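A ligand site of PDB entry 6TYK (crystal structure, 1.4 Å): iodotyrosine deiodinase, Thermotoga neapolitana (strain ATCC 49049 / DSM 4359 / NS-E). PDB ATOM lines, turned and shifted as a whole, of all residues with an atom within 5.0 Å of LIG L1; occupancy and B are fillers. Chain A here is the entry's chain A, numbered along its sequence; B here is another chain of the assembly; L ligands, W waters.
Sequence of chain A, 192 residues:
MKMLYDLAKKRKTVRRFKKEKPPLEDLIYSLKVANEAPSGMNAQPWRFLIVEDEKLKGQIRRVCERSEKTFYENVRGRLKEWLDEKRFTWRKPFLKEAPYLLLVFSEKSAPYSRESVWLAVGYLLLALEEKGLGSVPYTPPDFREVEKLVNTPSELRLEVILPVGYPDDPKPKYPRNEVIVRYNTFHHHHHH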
ATOM      1  N   ARG A  11      30.382  -4.508 -10.085  1.00  0.00           N
ATOM      2  CA  ARG A  11      31.019  -5.553  -9.306  1.00  0.00           C
ATOM      3  C   ARG A  11      29.995  -6.200  -8.366  1.00  0.00           C
ATOM      4  O   ARG A  11      29.251  -5.515  -7.671  1.00  0.00           O
ATOM      5  CB  ARG A  11      32.218  -5.003  -8.527  1.00  0.00           C
ATOM      6  CG  ARG A  11      33.106  -6.064  -7.930  1.00  0.00           C
ATOM      7  CD  ARG A  11      32.815  -6.288  -6.453  1.00  0.00           C
ATOM      8  NE  ARG A  11      33.343  -7.570  -5.999  1.00  0.00           N
ATOM      9  CZ  ARG A  11      32.719  -8.339  -5.115  1.00  0.00           C
ATOM     10  NH1 ARG A  11      31.576  -7.937  -4.581  1.00  0.00           N
ATOM     11  NH2 ARG A  11      33.248  -9.503  -4.757  1.00  0.00           N
ATOM     12  N   LYS A  12      29.961  -7.528  -8.386  1.00  0.00           N
ATOM     13  CA  LYS A  12      29.023  -8.272  -7.561  1.00  0.00           C
ATOM     14  C   LYS A  12      29.685  -9.561  -7.104  1.00  0.00           C
ATOM     15  O   LYS A  12      30.766  -9.921  -7.580  1.00  0.00           O
ATOM     16  CB  LYS A  12      27.770  -8.600  -8.354  1.00  0.00           C
ATOM     17  CG  LYS A  12      28.018  -9.459  -9.588  1.00  0.00           C
ATOM     18  CD  LYS A  12      26.713  -9.685 -10.321  1.00  0.00           C
ATOM     19  CE  LYS A  12      26.876 -10.603 -11.522  1.00  0.00           C
ATOM     20  NZ  LYS A  12      27.705 -10.012 -12.593  1.00  0.00           N
ATOM     21  N   THR A  13      29.049 -10.274  -6.185  1.00  0.00           N
ATOM     22  CA  THR A  13      29.623 -11.529  -5.715  1.00  0.00           C
ATOM     23  C   THR A  13      29.701 -12.519  -6.864  1.00  0.00           C
ATOM     24  O   THR A  13      28.801 -12.613  -7.700  1.00  0.00           O
ATOM     25  CB  THR A  13      28.750 -12.176  -4.630  1.00  0.00           C
ATOM     26  OG1 THR A  13      28.235 -11.180  -3.740  1.00  0.00           O
ATOM     27  CG2 THR A  13      29.584 -13.187  -3.849  1.00  0.00           C
ATOM     28  N   ARG A  15      30.219 -16.600  -6.994  1.00  0.00           N
ATOM     29  CA  ARG A  15      30.356 -17.860  -6.268  1.00  0.00           C
ATOM     30  C   ARG A  15      30.396 -19.022  -7.250  1.00  0.00           C
ATOM     31  O   ARG A  15      30.481 -20.174  -6.836  1.00  0.00           O
ATOM     32  CB  ARG A  15      29.187 -18.053  -5.297  1.00  0.00           C
ATOM     33  CG  ARG A  15      29.102 -16.972  -4.228  1.00  0.00           C
ATOM     34  CD  ARG A  15      27.899 -17.170  -3.318  1.00  0.00           C
ATOM     35  NE  ARG A  15      27.857 -16.181  -2.233  1.00  0.00           N
ATOM     36  CZ  ARG A  15      27.164 -15.048  -2.271  1.00  0.00           C
ATOM     37  NH1 ARG A  15      26.435 -14.748  -3.338  1.00  0.00           N
ATOM     38  NH2 ARG A  15      27.194 -14.234  -1.233  1.00  0.00           N
ATOM     39  N   GLU A  68      30.574 -24.820   8.420  1.00  0.00           N
ATOM     40  CA  GLU A  68      29.341 -24.258   7.897  1.00  0.00           C
ATOM     41  C   GLU A  68      28.144 -25.150   8.222  1.00  0.00           C
ATOM     42  O   GLU A  68      27.074 -24.657   8.549  1.00  0.00           O
ATOM     43  CB  GLU A  68      29.425 -24.046   6.378  1.00  0.00           C
ATOM     44  CG  GLU A  68      30.436 -23.002   5.929  1.00  0.00           C
ATOM     45  CD  GLU A  68      30.069 -21.584   6.332  1.00  0.00           C
ATOM     46  OE1 GLU A  68      29.112 -21.400   7.113  1.00  0.00           O
ATOM     47  OE2 GLU A  68      30.766 -20.666   5.867  1.00  0.00           O
ATOM     48  N   TRP A  82      17.976 -14.327   6.313  1.00  0.00           N
ATOM     49  CA  TRP A  82      18.550 -13.883   5.049  1.00  0.00           C
ATOM     50  C   TRP A  82      19.106 -15.063   4.253  1.00  0.00           C
ATOM     51  O   TRP A  82      18.858 -15.179   3.063  1.00  0.00           O
ATOM     52  CB  TRP A  82      19.633 -12.834   5.318  1.00  0.00           C
ATOM     53  CG  TRP A  82      20.204 -12.191   4.087  1.00  0.00           C
ATOM     54  CD1 TRP A  82      19.712 -11.099   3.436  1.00  0.00           C
ATOM     55  CD2 TRP A  82      21.414 -12.555   3.412  1.00  0.00           C
ATOM     56  NE1 TRP A  82      20.522 -10.778   2.371  1.00  0.00           N
ATOM     57  CE2 TRP A  82      21.576 -11.655   2.342  1.00  0.00           C
ATOM     58  CE3 TRP A  82      22.359 -13.560   3.595  1.00  0.00           C
ATOM     59  CZ2 TRP A  82      22.647 -11.728   1.455  1.00  0.00           C
ATOM     60  CZ3 TRP A  82      23.429 -13.637   2.721  1.00  0.00           C
ATOM     61  CH2 TRP A  82      23.567 -12.720   1.662  1.00  0.00           C
ATOM     62  N   PHE A  88      20.851 -20.201   0.657  1.00  0.00           N
ATOM     63  CA  PHE A  88      22.236 -20.565   0.922  1.00  0.00           C
ATOM     64  C   PHE A  88      22.302 -21.931   1.604  1.00  0.00           C
ATOM     65  O   PHE A  88      21.385 -22.304   2.338  1.00  0.00           O
ATOM     66  CB  PHE A  88      22.882 -19.534   1.845  1.00  0.00           C
ATOM     67  CG  PHE A  88      23.385 -18.293   1.151  1.00  0.00           C
ATOM     68  CD1 PHE A  88      22.506 -17.381   0.598  1.00  0.00           C
ATOM     69  CD2 PHE A  88      24.738 -18.023   1.110  1.00  0.00           C
ATOM     70  CE1 PHE A  88      22.978 -16.238  -0.019  1.00  0.00           C
ATOM     71  CE2 PHE A  88      25.200 -16.890   0.498  1.00  0.00           C
ATOM     72  CZ  PHE A  88      24.326 -15.997  -0.067  1.00  0.00           C
ATOM     73  N   LYS A  92      30.202 -25.663  -0.139  1.00  0.00           N
ATOM     74  CA  LYS A  92      30.987 -24.548  -0.683  1.00  0.00           C
ATOM     75  C   LYS A  92      31.798 -24.994  -1.900  1.00  0.00           C
ATOM     76  O   LYS A  92      33.031 -25.047  -1.850  1.00  0.00           O
ATOM     77  CB  LYS A  92      31.902 -23.962   0.390  1.00  0.00           C
ATOM     78  CG  LYS A  92      31.160 -23.358   1.583  1.00  0.00           C
ATOM     79  CD  LYS A  92      30.164 -22.283   1.159  1.00  0.00           C
ATOM     80  CE  LYS A  92      29.058 -22.069   2.204  1.00  0.00           C
ATOM     81  NZ  LYS A  92      27.928 -21.251   1.675  1.00  0.00           N
ATOM     82  N   PHE A  94      32.642 -23.474  -4.521  1.00  0.00           N
ATOM     83  CA  PHE A  94      33.601 -22.500  -5.055  1.00  0.00           C
ATOM     84  C   PHE A  94      34.992 -22.683  -4.462  1.00  0.00           C
ATOM     85  O   PHE A  94      35.979 -22.250  -5.054  1.00  0.00           O
ATOM     86  CB  PHE A  94      33.129 -21.054  -4.913  1.00  0.00           C
ATOM     87  CG  PHE A  94      32.727 -20.657  -3.522  1.00  0.00           C
ATOM     88  CD1 PHE A  94      33.679 -20.368  -2.571  1.00  0.00           C
ATOM     89  CD2 PHE A  94      31.398 -20.512  -3.197  1.00  0.00           C
ATOM     90  CE1 PHE A  94      33.306 -19.972  -1.281  1.00  0.00           C
ATOM     91  CE2 PHE A  94      31.016 -20.114  -1.922  1.00  0.00           C
ATOM     92  CZ  PHE A  94      31.971 -19.847  -0.968  1.00  0.00           C
ATOM     93  N   TRP A 118      40.975  -4.557   5.684  1.00  0.00           N
ATOM     94  CA  TRP A 118      39.668  -4.553   5.036  1.00  0.00           C
ATOM     95  C   TRP A 118      39.511  -3.411   4.048  1.00  0.00           C
ATOM     96  O   TRP A 118      38.934  -3.569   2.977  1.00  0.00           O
ATOM     97  CB  TRP A 118      38.536  -4.621   6.068  1.00  0.00           C
ATOM     98  CG  TRP A 118      38.395  -6.035   6.518  1.00  0.00           C
ATOM     99  CD1 TRP A 118      38.954  -6.622   7.609  1.00  0.00           C
ATOM    100  CD2 TRP A 118      37.704  -7.080   5.808  1.00  0.00           C
ATOM    101  NE1 TRP A 118      38.646  -7.973   7.636  1.00  0.00           N
ATOM    102  CE2 TRP A 118      37.869  -8.272   6.544  1.00  0.00           C
ATOM    103  CE3 TRP A 118      36.955  -7.116   4.622  1.00  0.00           C
ATOM    104  CZ2 TRP A 118      37.310  -9.478   6.144  1.00  0.00           C
ATOM    105  CZ3 TRP A 118      36.413  -8.305   4.226  1.00  0.00           C
ATOM    106  CH2 TRP A 118      36.583  -9.471   4.983  1.00  0.00           C
ATOM    107  N   VAL A 136      34.491 -13.612  -3.913  1.00  0.00           N
ATOM    108  CA  VAL A 136      33.530 -13.508  -2.823  1.00  0.00           C
ATOM    109  C   VAL A 136      34.361 -13.465  -1.544  1.00  0.00           C
ATOM    110  O   VAL A 136      35.284 -14.256  -1.375  1.00  0.00           O
ATOM    111  CB  VAL A 136      32.570 -14.715  -2.798  1.00  0.00           C
ATOM    112  CG1 VAL A 136      33.327 -16.035  -2.824  1.00  0.00           C
ATOM    113  CG2 VAL A 136      31.655 -14.648  -1.584  1.00  0.00           C
ATOM    114  N   PRO A 137      34.084 -12.493  -0.656  1.00  0.00           N
ATOM    115  CA  PRO A 137      34.798 -12.477   0.619  1.00  0.00           C
ATOM    116  C   PRO A 137      34.212 -13.557   1.509  1.00  0.00           C
ATOM    117  O   PRO A 137      33.202 -13.348   2.148  1.00  0.00           O
ATOM    118  CB  PRO A 137      34.472 -11.092   1.191  1.00  0.00           C
ATOM    119  CG  PRO A 137      33.907 -10.307   0.038  1.00  0.00           C
ATOM    120  CD  PRO A 137      33.212 -11.320  -0.809  1.00  0.00           C
ATOM    121  N   TYR A 138      34.830 -14.718   1.515  1.00  0.00           N
ATOM    122  CA  TYR A 138      34.297 -15.843   2.229  1.00  0.00           C
ATOM    123  C   TYR A 138      34.823 -15.882   3.657  1.00  0.00           C
ATOM    124  O   TYR A 138      36.036 -15.831   3.877  1.00  0.00           O
ATOM    125  CB  TYR A 138      34.593 -17.140   1.481  1.00  0.00           C
ATOM    126  CG  TYR A 138      34.126 -18.336   2.260  1.00  0.00           C
ATOM    127  CD1 TYR A 138      32.794 -18.455   2.615  1.00  0.00           C
ATOM    128  CD2 TYR A 138      35.024 -19.311   2.689  1.00  0.00           C
ATOM    129  CE1 TYR A 138      32.361 -19.518   3.356  1.00  0.00           C
ATOM    130  CE2 TYR A 138      34.591 -20.382   3.435  1.00  0.00           C
ATOM    131  CZ  TYR A 138      33.259 -20.481   3.766  1.00  0.00           C
ATOM    132  OH  TYR A 138      32.814 -21.540   4.514  1.00  0.00           O
ATOM    133  N   THR A 139      33.905 -15.907   4.607  1.00  0.00           N
ATOM    134  CA  THR A 139      34.258 -15.869   6.017  1.00  0.00           C
ATOM    135  C   THR A 139      33.609 -17.038   6.737  1.00  0.00           C
ATOM    136  O   THR A 139      32.469 -16.942   7.197  1.00  0.00           O
ATOM    137  CB  THR A 139      33.823 -14.534   6.659  1.00  0.00           C
ATOM    138  OG1 THR A 139      32.420 -14.349   6.451  1.00  0.00           O
ATOM    139  CG2 THR A 139      34.567 -13.370   6.030  1.00  0.00           C
ATOM    140  N   PRO A 140      34.328 -18.171   6.827  1.00  0.00           N
ATOM    141  CA  PRO A 140      33.788 -19.361   7.495  1.00  0.00           C
ATOM    142  C   PRO A 140      33.643 -19.107   8.994  1.00  0.00           C
ATOM    143  O   PRO A 140      34.235 -18.167   9.513  1.00  0.00           O
ATOM    144  CB  PRO A 140      34.859 -20.424   7.240  1.00  0.00           C
ATOM    145  CG  PRO A 140      36.130 -19.641   7.089  1.00  0.00           C
ATOM    146  CD  PRO A 140      35.724 -18.359   6.385  1.00  0.00           C
ATOM    147  N   PRO A 172      22.705 -12.443 -10.186  1.00  0.00           N
ATOM    148  CA  PRO A 172      22.653 -10.984 -10.225  1.00  0.00           C
ATOM    149  C   PRO A 172      23.020 -10.342  -8.893  1.00  0.00           C
ATOM    150  O   PRO A 172      22.858 -10.920  -7.818  1.00  0.00           O
ATOM    151  CB  PRO A 172      21.192 -10.691 -10.555  1.00  0.00           C
ATOM    152  CG  PRO A 172      20.709 -11.912 -11.240  1.00  0.00           C
ATOM    153  CD  PRO A 172      21.406 -13.038 -10.543  1.00  0.00           C
ATOM    154  N   LYS A 173      23.504  -9.107  -8.985  1.00  0.00           N
ATOM    155  CA  LYS A 173      23.810  -8.312  -7.815  1.00  0.00           C
ATOM    156  C   LYS A 173      22.545  -8.125  -6.995  1.00  0.00           C
ATOM    157  O   LYS A 173      21.448  -7.958  -7.551  1.00  0.00           O
ATOM    158  CB  LYS A 173      24.376  -6.964  -8.232  1.00  0.00           C
ATOM    159  CG  LYS A 173      25.049  -6.231  -7.089  1.00  0.00           C
ATOM    160  CD  LYS A 173      25.833  -5.014  -7.565  1.00  0.00           C
ATOM    161  CE  LYS A 173      26.466  -4.306  -6.380  1.00  0.00           C
ATOM    162  NZ  LYS A 173      27.518  -3.355  -6.777  1.00  0.00           N
ATOM    163  N   TYR A 174      22.672  -8.151  -5.670  1.00  0.00           N
ATOM    164  CA  TYR A 174      21.512  -7.877  -4.825  1.00  0.00           C
ATOM    165  C   TYR A 174      21.254  -6.373  -4.797  1.00  0.00           C
ATOM    166  O   TYR A 174      22.109  -5.589  -5.200  1.00  0.00           O
ATOM    167  CB  TYR A 174      21.739  -8.393  -3.410  1.00  0.00           C
ATOM    168  CG  TYR A 174      21.912  -9.886  -3.294  1.00  0.00           C
ATOM    169  CD1 TYR A 174      21.346 -10.769  -4.221  1.00  0.00           C
ATOM    170  CD2 TYR A 174      22.643 -10.439  -2.252  1.00  0.00           C
ATOM    171  CE1 TYR A 174      21.510 -12.138  -4.111  1.00  0.00           C
ATOM    172  CE2 TYR A 174      22.806 -11.802  -2.134  1.00  0.00           C
ATOM    173  CZ  TYR A 174      22.243 -12.648  -3.058  1.00  0.00           C
ATOM    174  OH  TYR A 174      22.425 -14.012  -2.924  1.00  0.00           O
ATOM    175  N   ARG A 176      20.617  -2.401  -3.643  1.00  0.00           N
ATOM    176  CA  ARG A 176      21.225  -1.470  -2.703  1.00  0.00           C
ATOM    177  C   ARG A 176      20.197  -0.448  -2.273  1.00  0.00           C
ATOM    178  O   ARG A 176      19.556   0.197  -3.107  1.00  0.00           O
ATOM    179  CB  ARG A 176      22.436  -0.762  -3.327  1.00  0.00           C
ATOM    180  CG  ARG A 176      23.627  -1.665  -3.611  1.00  0.00           C
ATOM    181  CD  ARG A 176      24.184  -2.275  -2.328  1.00  0.00           C
ATOM    182  NE  ARG A 176      25.472  -2.941  -2.513  1.00  0.00           N
ATOM    183  CZ  ARG A 176      25.603  -4.177  -2.984  1.00  0.00           C
ATOM    184  NH1 ARG A 176      24.525  -4.880  -3.343  1.00  0.00           N
ATOM    185  NH2 ARG A 176      26.803  -4.716  -3.084  1.00  0.00           N
ATOM    186  N   GLU B  36      27.904   0.920  -3.120  1.00  0.00           N
ATOM    187  CA  GLU B  36      27.873  -0.202  -4.044  1.00  0.00           C
ATOM    188  C   GLU B  36      28.757  -1.354  -3.594  1.00  0.00           C
ATOM    189  O   GLU B  36      28.742  -2.433  -4.186  1.00  0.00           O
ATOM    190  CB  GLU B  36      28.305   0.250  -5.445  1.00  0.00           C
ATOM    191  CG  GLU B  36      27.294   1.118  -6.160  1.00  0.00           C
ATOM    192  CD  GLU B  36      25.986   0.381  -6.385  1.00  0.00           C
ATOM    193  OE1 GLU B  36      26.016  -0.857  -6.613  1.00  0.00           O
ATOM    194  OE2 GLU B  36      24.924   1.033  -6.317  1.00  0.00           O
ATOM    195  N   PRO B  38      30.282  -4.519  -1.450  1.00  0.00           N
ATOM    196  CA  PRO B  38      29.705  -5.673  -0.774  1.00  0.00           C
ATOM    197  C   PRO B  38      29.680  -5.476   0.744  1.00  0.00           C
ATOM    198  O   PRO B  38      30.348  -4.574   1.265  1.00  0.00           O
ATOM    199  CB  PRO B  38      30.672  -6.788  -1.135  1.00  0.00           C
ATOM    200  CG  PRO B  38      31.979  -6.097  -1.307  1.00  0.00           C
ATOM    201  CD  PRO B  38      31.630  -4.804  -1.983  1.00  0.00           C
ATOM    202  N   SER B  39      28.908  -6.299   1.434  1.00  0.00           N
ATOM    203  CA  SER B  39      28.847  -6.232   2.883  1.00  0.00           C
ATOM    204  C   SER B  39      28.268  -7.538   3.390  1.00  0.00           C
ATOM    205  O   SER B  39      27.552  -8.221   2.658  1.00  0.00           O
ATOM    206  CB  SER B  39      28.020  -5.030   3.358  1.00  0.00           C
ATOM    207  OG  SER B  39      26.680  -5.117   2.911  1.00  0.00           O
ATOM    208  N   GLY B  40      28.577  -7.903   4.633  1.00  0.00           N
ATOM    209  CA  GLY B  40      28.007  -9.114   5.215  1.00  0.00           C
ATOM    210  C   GLY B  40      26.485  -9.072   5.120  1.00  0.00           C
ATOM    211  O   GLY B  40      25.863  -8.067   5.454  1.00  0.00           O
ATOM    212  N   MET B  41      25.906 -10.183   4.647  1.00  0.00           N
ATOM    213  CA  MET B  41      24.469 -10.324   4.358  1.00  0.00           C
ATOM    214  C   MET B  41      23.825  -9.133   3.644  1.00  0.00           C
ATOM    215  O   MET B  41      22.643  -8.871   3.807  1.00  0.00           O
ATOM    216  CB  MET B  41      23.657 -10.777   5.573  1.00  0.00           C
ATOM    217  CG  MET B  41      23.519  -9.811   6.750  1.00  0.00           C
ATOM    218  SD  MET B  41      22.167 -10.339   7.879  1.00  0.00           S
ATOM    219  CE  MET B  41      20.739  -9.843   6.901  1.00  0.00           C
ATOM    220  N   ASN B  42      24.622  -8.465   2.816  1.00  0.00           N
ATOM    221  CA  ASN B  42      24.169  -7.272   2.111  1.00  0.00           C
ATOM    222  C   ASN B  42      23.467  -6.265   3.032  1.00  0.00           C
ATOM    223  O   ASN B  42      22.560  -5.567   2.615  1.00  0.00           O
ATOM    224  CB  ASN B  42      23.278  -7.628   0.927  1.00  0.00           C
ATOM    225  CG  ASN B  42      23.095  -6.469  -0.030  1.00  0.00           C
ATOM    226  OD1 ASN B  42      24.000  -5.661  -0.214  1.00  0.00           O
ATOM    227  ND2 ASN B  42      21.929  -6.365  -0.618  1.00  0.00           N
ATOM    228  N   TYR B 112      29.591  -8.966  10.416  1.00  0.00           N
ATOM    229  CA  TYR B 112      30.790  -8.434   9.777  1.00  0.00           C
ATOM    230  C   TYR B 112      30.629  -6.956   9.424  1.00  0.00           C
ATOM    231  O   TYR B 112      31.147  -6.475   8.399  1.00  0.00           O
ATOM    232  CB  TYR B 112      31.164  -9.256   8.543  1.00  0.00           C
ATOM    233  CG  TYR B 112      31.926 -10.501   8.922  1.00  0.00           C
ATOM    234  CD1 TYR B 112      31.266 -11.640   9.349  1.00  0.00           C
ATOM    235  CD2 TYR B 112      33.314 -10.521   8.885  1.00  0.00           C
ATOM    236  CE1 TYR B 112      31.972 -12.777   9.723  1.00  0.00           C
ATOM    237  CE2 TYR B 112      34.028 -11.647   9.254  1.00  0.00           C
ATOM    238  CZ  TYR B 112      33.347 -12.772   9.670  1.00  0.00           C
ATOM    239  OH  TYR B 112      34.032 -13.912  10.041  1.00  0.00           O
ATOM    240  N   GLU B 115      34.148  -4.897   9.387  1.00  0.00           N
ATOM    241  CA  GLU B 115      34.887  -5.292   8.209  1.00  0.00           C
ATOM    242  C   GLU B 115      34.261  -4.707   6.954  1.00  0.00           C
ATOM    243  O   GLU B 115      34.948  -4.215   6.071  1.00  0.00           O
ATOM    244  CB  GLU B 115      34.943  -6.819   8.101  1.00  0.00           C
ATOM    245  CG  GLU B 115      35.712  -7.479   9.249  1.00  0.00           C
ATOM    246  CD  GLU B 115      34.838  -7.856  10.444  1.00  0.00           C
ATOM    247  OE1 GLU B 115      33.722  -7.303  10.609  1.00  0.00           O
ATOM    248  OE2 GLU B 115      35.274  -8.722  11.221  1.00  0.00           O
ATOM    249  N   SER B 116      32.940  -4.785   6.861  1.00  0.00           N
ATOM    250  CA  SER B 116      32.242  -4.304   5.679  1.00  0.00           C
ATOM    251  C   SER B 116      32.354  -2.786   5.516  1.00  0.00           C
ATOM    252  O   SER B 116      32.530  -2.286   4.408  1.00  0.00           O
ATOM    253  CB  SER B 116      30.763  -4.682   5.738  1.00  0.00           C
ATOM    254  OG  SER B 116      30.583  -6.093   5.800  1.00  0.00           O
ATOM    255  N   LEU B 119      35.875  -1.986   4.290  1.00  0.00           N
ATOM    256  CA  LEU B 119      35.961  -2.303   2.890  1.00  0.00           C
ATOM    257  C   LEU B 119      35.341  -1.150   2.073  1.00  0.00           C
ATOM    258  O   LEU B 119      35.926  -0.668   1.095  1.00  0.00           O
ATOM    259  CB  LEU B 119      35.233  -3.628   2.650  1.00  0.00           C
ATOM    260  CG  LEU B 119      35.340  -4.297   1.289  1.00  0.00           C
ATOM    261  CD1 LEU B 119      34.939  -5.762   1.415  1.00  0.00           C
ATOM    262  CD2 LEU B 119      34.475  -3.597   0.240  1.00  0.00           C
HETATM  263  N1  LIG L   1      29.319 -14.428   1.045  1.00  0.00           N
HETATM  264  C1  LIG L   1      29.223 -15.764   1.290  1.00  0.00           C
HETATM  265  O1  LIG L   1      28.673 -16.488   0.483  1.00  0.00           O
HETATM  266  N2  LIG L   1      29.762 -16.308   2.435  1.00  0.00           N
HETATM  267  C2  LIG L   1      30.372 -15.513   3.363  1.00  0.00           C
HETATM  268  O2  LIG L   1      30.844 -16.025   4.382  1.00  0.00           O
HETATM  269  C3  LIG L   1      30.483 -14.144   3.113  1.00  0.00           C
HETATM  270  N3  LIG L   1      31.111 -13.318   4.014  1.00  0.00           N
HETATM  271  C4  LIG L   1      31.237 -11.963   3.739  1.00  0.00           C
HETATM  272  C5  LIG L   1      31.897 -11.148   4.653  1.00  0.00           C
HETATM  273  C6  LIG L   1      32.049  -9.790   4.416  1.00  0.00           C
HETATM  274  C7  LIG L   1      32.777  -8.951   5.434  1.00  0.00           C
HETATM  275  C8  LIG L   1      31.523  -9.246   3.250  1.00  0.00           C
HETATM  276  C9  LIG L   1      31.672  -7.774   2.968  1.00  0.00           C
HETATM  277  C10 LIG L   1      30.863 -10.060   2.336  1.00  0.00           C
HETATM  278  C11 LIG L   1      30.712 -11.427   2.578  1.00  0.00           C
HETATM  279  N4  LIG L   1      30.033 -12.256   1.682  1.00  0.00           N
HETATM  280  C12 LIG L   1      29.960 -13.610   1.930  1.00  0.00           C
HETATM  281  C13 LIG L   1      29.445 -11.712   0.411  1.00  0.00           C
HETATM  282  C14 LIG L   1      28.116 -10.979   0.712  1.00  0.00           C
HETATM  283  O3  LIG L   1      27.061 -11.894   0.958  1.00  0.00           O
HETATM  284  C15 LIG L   1      27.792 -10.040  -0.443  1.00  0.00           C
HETATM  285  O4  LIG L   1      28.786  -9.038  -0.480  1.00  0.00           O
HETATM  286  C16 LIG L   1      26.411  -9.387  -0.338  1.00  0.00           C
HETATM  287  O5  LIG L   1      25.399 -10.387  -0.446  1.00  0.00           O
HETATM  288  C17 LIG L   1      26.210  -8.357  -1.443  1.00  0.00           C
HETATM  289  O6  LIG L   1      26.440  -8.965  -2.689  1.00  0.00           O
HETATM  290  P1  LIG L   1      26.284  -8.145  -4.062  1.00  0.00           P
HETATM  291  O7  LIG L   1      26.479  -9.194  -5.155  1.00  0.00           O
HETATM  292  O8  LIG L   1      27.392  -7.134  -4.144  1.00  0.00           O
HETATM  293  O9  LIG L   1      24.893  -7.550  -4.089  1.00  0.00           O
HETATM  294  N1  LG2 L   2      29.566 -18.078   5.782  1.00  0.00           N
HETATM  295  C1  LG2 L   2      28.249 -18.611   5.526  1.00  0.00           C
HETATM  296  C2  LG2 L   2      27.063 -17.668   5.798  1.00  0.00           C
HETATM  297  C3  LG2 L   2      27.147 -16.319   5.177  1.00  0.00           C
HETATM  298  C4  LG2 L   2      27.562 -15.228   5.951  1.00  0.00           C
HETATM  299  C5  LG2 L   2      27.625 -13.931   5.440  1.00  0.00           C
HETATM  300  I1  LG2 L   2      28.278 -12.447   6.634  1.00  0.00           I
HETATM  301  C6  LG2 L   2      27.256 -13.719   4.113  1.00  0.00           C
HETATM  302  O1  LG2 L   2      27.284 -12.484   3.527  1.00  0.00           O
HETATM  303  C7  LG2 L   2      26.842 -14.795   3.306  1.00  0.00           C
HETATM  304  C8  LG2 L   2      26.774 -16.077   3.842  1.00  0.00           C
HETATM  305  C9  LG2 L   2      28.089 -19.099   4.103  1.00  0.00           C
HETATM  306  O2  LG2 L   2      27.163 -19.736   3.614  1.00  0.00           O
HETATM  307  O3  LG2 L   2      29.134 -18.788   3.286  1.00  0.00           O
HETATM  308  O   HOH W   1      24.766 -11.163  -5.525  1.00  0.00           O
HETATM  309  O   HOH W   2      25.851 -11.967  -2.780  1.00  0.00           O
HETATM  310  O   HOH W   3      29.680  -5.844  -4.774  1.00  0.00           O
HETATM  311  O   HOH W   4      28.111 -19.072   0.016  1.00  0.00           O
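N of Tyr 174 is in hydrogen-bond range of O9 of LIG L1. The side-chain carboxylate (OE2) of Glu 68 is in salt-bridge range of a nitrogen (N1) of LG2 L2. The backbone NH (N) of Thr 139 sits at hydrogen-bond distance from an oxygen (O2) of LIG L1. An oxygen (O8) of LIG L1 lies within salt-bridge range of the guanidinium group (NH2) of Arg 176. NE of Arg 15 lies within hydrogen-bond range of O1 of LIG L1 (2.9 Å). N of Ser 39 of chain B lies within hydrogen-bond range of O4 of LIG L1, 3.3 Å away. The side-chain hydroxyl (OG1) of Thr 13 sits at hydrogen-bond distance from an oxygen (O7) of LIG L1, 3.0 Å away. The side-chain hydroxyl (OG1) of Thr 139 is in hydrogen-bond range of a nitrogen (N3) of LIG L1. A nitrogen (N1) of LG2 L2 is in hydrogen-bond range of the backbone carbonyl oxygen (O) of Thr 139, at 3.4 Å. The backbone NH (N) of Met 41 of chain B lies within hydrogen-bond range of an oxygen (O1) of LG2 L2 (2.9 Å). O2 of LG2 L2 lies within salt-bridge range of NZ of Lys 92 (2.6 Å). O7 of LIG L1 is in hydrogen-bond range of N of Thr 13 (3.0 Å). An oxygen (O4) of LIG L1 sits close to the backbone carbonyl oxygen (O) of Ser 39 of chain B (3.5 Å).
O3 of LIG L1 sits at hydrogen-bond distance from O1 of LG2 L2 (2.6 Å).
O of Met 41 of chain B is in hydrogen-bond range of NE1 of Trp 82 (3.2 Å). NH2 of Arg 176 sits at hydrogen-bond distance from O of Glu 36 of chain B (3.2 Å). OG of Ser 116 of chain B is in hydrogen-bond range of N of Gly 40 of chain B. The guanidinium group (NH1) of Arg 176 sits at hydrogen-bond distance from the backbone carbonyl oxygen (O) of Tyr 174. The side-chain amino group (NZ) of Lys 173 is in salt-bridge range of the side-chain carboxylate (OE1) of Glu 36 of chain B (2.9 Å). NZ of Lys 173 sits at hydrogen-bond distance from O of Arg 11. The side-chain hydroxyl (OH) of Tyr 138 lies within hydrogen-bond range of the side-chain carboxylate (OE2) of Glu 68, at 2.6 Å. OG of Ser 116 of chain B lies within hydrogen-bond range of O of Tyr 112 of chain B.
N3 of LIG L1 sits close to O of Pro 137 (2.8 Å). Merely in contact with LIG L1: Lys 12, Trp 82, Phe 88, Trp 118, Val 136, Tyr 138, Lys 173, Pro 38 of chain B, Gly 40 of chain B, Asn 42 of chain B, Tyr 112 of chain B and Ser 116 of chain B. Along chain A the residues within 4 Å of LIG L1 span positions 12 to 176.
Water W1 bridges an oxygen (O7) of LIG L1 and the backbone carbonyl oxygen of Pro 172. Water W4 lies within hydrogen-bond range of an oxygen (O1) of LIG L1, the side-chain amino group of Lys 92 and an oxygen (O3) of LG2 L2. Water W3 bridges an oxygen (O8) of LIG L1 (2.7 Å) and the guanidinium group (NH1) of Arg 11 (2.8 Å). Water W2 lies within hydrogen-bond range of OG1 of Thr 13 (2.7 Å), O5 of LIG L1 (2.9 Å) and NH1 of Arg 15 (2.9 Å).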
